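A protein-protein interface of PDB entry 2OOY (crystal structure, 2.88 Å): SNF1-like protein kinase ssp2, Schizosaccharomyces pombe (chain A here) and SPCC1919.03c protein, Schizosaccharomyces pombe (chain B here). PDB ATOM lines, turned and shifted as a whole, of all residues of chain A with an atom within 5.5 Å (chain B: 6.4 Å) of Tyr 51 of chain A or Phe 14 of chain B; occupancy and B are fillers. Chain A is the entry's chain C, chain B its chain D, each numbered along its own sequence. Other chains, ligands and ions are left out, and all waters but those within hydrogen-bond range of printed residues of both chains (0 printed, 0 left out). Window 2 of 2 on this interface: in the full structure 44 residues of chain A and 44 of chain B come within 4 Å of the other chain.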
ATOM      1  N   VAL A  43      -2.632 -17.351 -16.564  1.00  0.00           N
ATOM      2  CA  VAL A  43      -3.141 -18.102 -17.716  1.00  0.00           C
ATOM      3  C   VAL A  43      -4.496 -18.710 -17.323  1.00  0.00           C
ATOM      4  O   VAL A  43      -4.748 -18.996 -16.139  1.00  0.00           O
ATOM      5  CB  VAL A  43      -2.177 -19.270 -18.091  1.00  0.00           C
ATOM      6  CG1 VAL A  43      -2.746 -20.183 -19.233  1.00  0.00           C
ATOM      7  CG2 VAL A  43      -0.793 -18.742 -18.465  1.00  0.00           C
ATOM      8  N   PRO A  44      -5.394 -18.866 -18.306  1.00  0.00           N
ATOM      9  CA  PRO A  44      -6.646 -19.616 -18.237  1.00  0.00           C
ATOM     10  C   PRO A  44      -6.717 -20.865 -17.315  1.00  0.00           C
ATOM     11  O   PRO A  44      -5.707 -21.543 -17.068  1.00  0.00           O
ATOM     12  CB  PRO A  44      -6.875 -19.989 -19.693  1.00  0.00           C
ATOM     13  CG  PRO A  44      -6.457 -18.753 -20.391  1.00  0.00           C
ATOM     14  CD  PRO A  44      -5.281 -18.195 -19.610  1.00  0.00           C
ATOM     15  N   LYS A  45      -7.926 -21.127 -16.805  1.00  0.00           N
ATOM     16  CA  LYS A  45      -8.157 -22.240 -15.890  1.00  0.00           C
ATOM     17  C   LYS A  45      -9.115 -23.212 -16.572  1.00  0.00           C
ATOM     18  O   LYS A  45     -10.324 -22.933 -16.665  1.00  0.00           O
ATOM     19  CB  LYS A  45      -8.747 -21.744 -14.563  1.00  0.00           C
ATOM     20  CG  LYS A  45      -8.093 -20.462 -13.993  1.00  0.00           C
ATOM     21  CD  LYS A  45      -6.608 -20.647 -13.639  1.00  0.00           C
ATOM     22  CE  LYS A  45      -6.433 -21.604 -12.462  1.00  0.00           C
ATOM     23  NZ  LYS A  45      -7.017 -22.967 -12.739  1.00  0.00           N
ATOM     24  N   PRO A  46      -8.571 -24.323 -17.108  1.00  0.00           N
ATOM     25  CA  PRO A  46      -9.421 -25.351 -17.685  1.00  0.00           C
ATOM     26  C   PRO A  46     -10.095 -26.107 -16.565  1.00  0.00           C
ATOM     27  O   PRO A  46      -9.439 -26.562 -15.613  1.00  0.00           O
ATOM     28  CB  PRO A  46      -8.449 -26.253 -18.448  1.00  0.00           C
ATOM     29  CG  PRO A  46      -7.106 -25.569 -18.404  1.00  0.00           C
ATOM     30  CD  PRO A  46      -7.141 -24.657 -17.221  1.00  0.00           C
ATOM     31  N   VAL A  47     -11.414 -26.195 -16.670  1.00  0.00           N
ATOM     32  CA  VAL A  47     -12.219 -26.873 -15.662  1.00  0.00           C
ATOM     33  C   VAL A  47     -13.050 -27.985 -16.345  1.00  0.00           C
ATOM     34  O   VAL A  47     -14.074 -27.739 -16.995  1.00  0.00           O
ATOM     35  CB  VAL A  47     -12.980 -25.837 -14.738  1.00  0.00           C
ATOM     36  CG1 VAL A  47     -14.219 -26.438 -14.042  1.00  0.00           C
ATOM     37  CG2 VAL A  47     -11.999 -25.240 -13.698  1.00  0.00           C
ATOM     38  N   GLY A  49     -13.641 -30.730 -19.211  1.00  0.00           N
ATOM     39  CA  GLY A  49     -13.549 -30.506 -20.686  1.00  0.00           C
ATOM     40  C   GLY A  49     -13.195 -29.042 -21.002  1.00  0.00           C
ATOM     41  O   GLY A  49     -13.960 -28.301 -21.667  1.00  0.00           O
ATOM     42  N   LYS A  50     -12.054 -28.626 -20.450  1.00  0.00           N
ATOM     43  CA  LYS A  50     -11.404 -27.339 -20.727  1.00  0.00           C
ATOM     44  C   LYS A  50     -11.931 -26.065 -20.074  1.00  0.00           C
ATOM     45  O   LYS A  50     -12.157 -25.983 -18.868  1.00  0.00           O
ATOM     46  CB  LYS A  50     -11.224 -27.130 -22.253  1.00  0.00           C
ATOM     47  N   TYR A  51     -12.117 -25.073 -20.927  1.00  0.00           N
ATOM     48  CA  TYR A  51     -11.874 -23.699 -20.534  1.00  0.00           C
ATOM     49  C   TYR A  51     -13.103 -22.932 -20.090  1.00  0.00           C
ATOM     50  O   TYR A  51     -14.176 -23.087 -20.660  1.00  0.00           O
ATOM     51  CB  TYR A  51     -11.115 -22.951 -21.648  1.00  0.00           C
ATOM     52  CG  TYR A  51      -9.640 -23.262 -21.655  1.00  0.00           C
ATOM     53  CD1 TYR A  51      -9.018 -23.830 -22.775  1.00  0.00           C
ATOM     54  CD2 TYR A  51      -8.866 -23.013 -20.527  1.00  0.00           C
ATOM     55  CE1 TYR A  51      -7.644 -24.130 -22.768  1.00  0.00           C
ATOM     56  CE2 TYR A  51      -7.502 -23.302 -20.507  1.00  0.00           C
ATOM     57  CZ  TYR A  51      -6.896 -23.862 -21.618  1.00  0.00           C
ATOM     58  OH  TYR A  51      -5.536 -24.113 -21.557  1.00  0.00           O
ATOM     59  N   ARG A  52     -12.926 -22.095 -19.076  1.00  0.00           N
ATOM     60  CA  ARG A  52     -14.024 -21.277 -18.611  1.00  0.00           C
ATOM     61  C   ARG A  52     -14.025 -19.832 -19.180  1.00  0.00           C
ATOM     62  O   ARG A  52     -13.026 -19.310 -19.702  1.00  0.00           O
ATOM     63  CB  ARG A  52     -14.091 -21.295 -17.078  1.00  0.00           C
ATOM     64  N   SER A  53     -15.191 -19.212 -19.105  1.00  0.00           N
ATOM     65  CA  SER A  53     -15.317 -17.793 -19.303  1.00  0.00           C
ATOM     66  C   SER A  53     -14.480 -17.039 -18.264  1.00  0.00           C
ATOM     67  O   SER A  53     -14.112 -15.880 -18.484  1.00  0.00           O
ATOM     68  CB  SER A  53     -16.774 -17.442 -19.178  1.00  0.00           C
ATOM     69  OG  SER A  53     -17.501 -18.576 -19.611  1.00  0.00           O
ATOM     70  N   MET A  55     -11.646 -17.195 -18.249  1.00  0.00           N
ATOM     71  CA  MET A  55     -10.369 -16.967 -18.950  1.00  0.00           C
ATOM     72  C   MET A  55     -10.185 -15.523 -19.340  1.00  0.00           C
ATOM     73  O   MET A  55      -9.055 -15.064 -19.468  1.00  0.00           O
ATOM     74  CB  MET A  55     -10.160 -17.882 -20.177  1.00  0.00           C
ATOM     75  CG  MET A  55     -11.150 -17.717 -21.317  1.00  0.00           C
ATOM     76  SD  MET A  55     -10.685 -18.927 -22.506  1.00  0.00           S
ATOM     77  CE  MET A  55     -11.436 -18.339 -24.020  1.00  0.00           C
ATOM     78  N   ILE B  11       2.481 -16.504 -22.611  1.00  0.00           N
ATOM     79  CA  ILE B  11       1.190 -16.599 -23.261  1.00  0.00           C
ATOM     80  C   ILE B  11       0.776 -18.044 -23.451  1.00  0.00           C
ATOM     81  O   ILE B  11       1.545 -18.843 -23.949  1.00  0.00           O
ATOM     82  CB  ILE B  11       1.120 -15.745 -24.587  1.00  0.00           C
ATOM     83  CG1 ILE B  11       0.403 -16.470 -25.730  1.00  0.00           C
ATOM     84  CG2 ILE B  11       2.482 -15.325 -25.045  1.00  0.00           C
ATOM     85  CD1 ILE B  11      -1.091 -16.377 -25.701  1.00  0.00           C
ATOM     86  N   PRO B  12      -0.437 -18.390 -23.008  1.00  0.00           N
ATOM     87  CA  PRO B  12      -0.998 -19.737 -23.129  1.00  0.00           C
ATOM     88  C   PRO B  12      -0.819 -20.294 -24.525  1.00  0.00           C
ATOM     89  O   PRO B  12      -0.861 -19.542 -25.494  1.00  0.00           O
ATOM     90  CB  PRO B  12      -2.483 -19.528 -22.844  1.00  0.00           C
ATOM     91  CG  PRO B  12      -2.518 -18.389 -21.958  1.00  0.00           C
ATOM     92  CD  PRO B  12      -1.358 -17.489 -22.306  1.00  0.00           C
ATOM     93  N   ALA B  13      -0.619 -21.604 -24.608  1.00  0.00           N
ATOM     94  CA  ALA B  13      -0.254 -22.208 -25.867  1.00  0.00           C
ATOM     95  C   ALA B  13      -1.391 -22.064 -26.895  1.00  0.00           C
ATOM     96  O   ALA B  13      -1.167 -21.626 -28.028  1.00  0.00           O
ATOM     97  CB  ALA B  13       0.155 -23.680 -25.663  1.00  0.00           C
ATOM     98  N   PHE B  14      -2.609 -22.397 -26.482  1.00  0.00           N
ATOM     99  CA  PHE B  14      -3.729 -22.491 -27.414  1.00  0.00           C
ATOM    100  C   PHE B  14      -4.070 -21.143 -28.062  1.00  0.00           C
ATOM    101  O   PHE B  14      -4.330 -21.063 -29.269  1.00  0.00           O
ATOM    102  CB  PHE B  14      -4.954 -23.120 -26.721  1.00  0.00           C
ATOM    103  CG  PHE B  14      -5.415 -22.361 -25.516  1.00  0.00           C
ATOM    104  CD1 PHE B  14      -4.707 -22.451 -24.299  1.00  0.00           C
ATOM    105  CD2 PHE B  14      -6.536 -21.519 -25.599  1.00  0.00           C
ATOM    106  CE1 PHE B  14      -5.118 -21.712 -23.184  1.00  0.00           C
ATOM    107  CE2 PHE B  14      -6.966 -20.781 -24.491  1.00  0.00           C
ATOM    108  CZ  PHE B  14      -6.261 -20.870 -23.284  1.00  0.00           C
ATOM    109  N   LEU B  15      -4.043 -20.089 -27.256  1.00  0.00           N
ATOM    110  CA  LEU B  15      -4.295 -18.750 -27.739  1.00  0.00           C
ATOM    111  C   LEU B  15      -3.331 -18.393 -28.841  1.00  0.00           C
ATOM    112  O   LEU B  15      -3.711 -17.667 -29.747  1.00  0.00           O
ATOM    113  CB  LEU B  15      -4.134 -17.723 -26.627  1.00  0.00           C
ATOM    114  CG  LEU B  15      -5.110 -17.688 -25.458  1.00  0.00           C
ATOM    115  CD1 LEU B  15      -4.773 -16.522 -24.578  1.00  0.00           C
ATOM    116  CD2 LEU B  15      -6.515 -17.535 -25.946  1.00  0.00           C
ATOM    117  N   THR B  16      -2.095 -18.901 -28.760  1.00  0.00           N
ATOM    118  CA  THR B  16      -1.021 -18.427 -29.636  1.00  0.00           C
ATOM    119  C   THR B  16      -1.400 -18.644 -31.095  1.00  0.00           C
ATOM    120  O   THR B  16      -2.275 -17.942 -31.606  1.00  0.00           O
ATOM    121  CB  THR B  16       0.451 -18.939 -29.303  1.00  0.00           C
ATOM    122  OG1 THR B  16       0.595 -20.307 -29.662  1.00  0.00           O
ATOM    123  CG2 THR B  16       0.805 -18.821 -27.855  1.00  0.00           C
ATOM    124  N   SER B  17      -0.780 -19.618 -31.758  1.00  0.00           N
ATOM    125  CA  SER B  17      -0.681 -19.607 -33.240  1.00  0.00           C
ATOM    126  C   SER B  17      -1.958 -19.862 -34.047  1.00  0.00           C
ATOM    127  O   SER B  17      -3.075 -19.479 -33.662  1.00  0.00           O
ATOM    128  CB  SER B  17       0.480 -20.516 -33.749  1.00  0.00           C
ATOM    129  OG  SER B  17       0.203 -21.917 -33.609  1.00  0.00           O
ATOM    130  N   THR B  19      -4.952 -21.187 -36.819  1.00  0.00           N
ATOM    131  CA  THR B  19      -6.211 -21.740 -36.370  1.00  0.00           C
ATOM    132  C   THR B  19      -6.190 -21.714 -34.833  1.00  0.00           C
ATOM    133  O   THR B  19      -6.300 -22.746 -34.166  1.00  0.00           O
ATOM    134  CB  THR B  19      -6.559 -23.107 -37.037  1.00  0.00           C
ATOM    135  OG1 THR B  19      -6.864 -22.869 -38.417  1.00  0.00           O
ATOM    136  CG2 THR B  19      -7.778 -23.799 -36.379  1.00  0.00           C
ATOM    137  N   LEU B  20      -5.982 -20.505 -34.296  1.00  0.00           N
ATOM    138  CA  LEU B  20      -6.440 -20.154 -32.945  1.00  0.00           C
ATOM    139  C   LEU B  20      -7.956 -20.116 -32.984  1.00  0.00           C
ATOM    140  O   LEU B  20      -8.605 -20.207 -31.941  1.00  0.00           O
ATOM    141  CB  LEU B  20      -5.896 -18.786 -32.490  1.00  0.00           C
ATOM    142  CG  LEU B  20      -6.466 -17.948 -31.315  1.00  0.00           C
ATOM    143  CD1 LEU B  20      -7.655 -17.071 -31.731  1.00  0.00           C
ATOM    144  CD2 LEU B  20      -6.797 -18.784 -30.081  1.00  0.00           C
ATOM    145  N   LEU B  23     -10.838 -25.244 -31.218  1.00  0.00           N
ATOM    146  CA  LEU B  23     -11.734 -25.967 -30.253  1.00  0.00           C
ATOM    147  C   LEU B  23     -12.123 -25.368 -28.915  1.00  0.00           C
ATOM    148  O   LEU B  23     -11.514 -25.656 -27.871  1.00  0.00           O
ATOM    149  CB  LEU B  23     -11.472 -27.486 -30.121  1.00  0.00           C
ATOM    150  CG  LEU B  23     -12.730 -28.325 -29.734  1.00  0.00           C
ATOM    151  CD1 LEU B  23     -12.658 -29.042 -28.350  1.00  0.00           C
ATOM    152  CD2 LEU B  23     -14.094 -27.569 -29.932  1.00  0.00           C
ATOM    153  N   LYS B  24     -13.162 -24.534 -29.026  1.00  0.00           N
ATOM    154  CA  LYS B  24     -14.088 -24.121 -27.960  1.00  0.00           C
ATOM    155  C   LYS B  24     -14.701 -22.728 -28.299  1.00  0.00           C
ATOM    156  O   LYS B  24     -15.232 -22.559 -29.409  1.00  0.00           O
ATOM    157  CB  LYS B  24     -13.490 -24.263 -26.534  1.00  0.00           C
ATOM    158  CG  LYS B  24     -12.733 -23.044 -25.950  1.00  0.00           C
ATOM    159  CD  LYS B  24     -11.488 -22.621 -26.738  1.00  0.00           C
ATOM    160  CE  LYS B  24     -11.134 -21.185 -26.421  1.00  0.00           C
ATOM    161  NZ  LYS B  24     -12.247 -20.275 -26.785  1.00  0.00           N
ATOM    162  N   PRO B  26     -15.381 -20.277 -24.899  1.00  0.00           N
ATOM    163  CA  PRO B  26     -16.061 -19.650 -23.772  1.00  0.00           C
ATOM    164  C   PRO B  26     -16.140 -18.181 -24.159  1.00  0.00           C
ATOM    165  O   PRO B  26     -15.190 -17.651 -24.767  1.00  0.00           O
ATOM    166  CB  PRO B  26     -15.089 -19.830 -22.612  1.00  0.00           C
ATOM    167  CG  PRO B  26     -14.195 -20.925 -23.036  1.00  0.00           C
ATOM    168  CD  PRO B  26     -14.097 -20.872 -24.504  1.00  0.00           C
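Among the printed residues, merely in contact across the chains: Val 43 of chain A with Pro 12 of chain B, Pro 44 of chain A with Pro 12 of chain B, Pro 44 of chain A with Phe 14 of chain B, Tyr 51 of chain A with Phe 14 of chain B, Tyr 51 of chain A with Pro 26 of chain B, Arg 52 of chain A with Pro 26 of chain B, Ser 53 of chain A with Pro 26 of chain B, Met 55 of chain A with Lys 24 of chain B and Met 55 of chain A with Pro 26 of chain B.
Of chain B, only Phe 14 and Pro 26 come within 4 Å of Tyr 51 of chain A.
Of the printed residues of chain B, Ser 53 of chain A touches Pro 26 (3.6 Å).
Of the printed residues of chain A, Pro 12 of chain B touches Val 43 (3.3 Å) and Pro 44 (3.6 Å).
Phe 14 of chain B touches two residues of chain A.
The nearest residue of chain B that does not touch Tyr 51 of chain A is Lys 24 of chain B (4.6 Å).
Of the 12 printed residues of chain B, 4 touch a printed residue of chain A.
Printed residues of chain B that touch a printed residue of chain A: Pro 12, Phe 14, Lys 24 and Pro 26.
Among the printed residues, 9 pairs touch across the chains.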
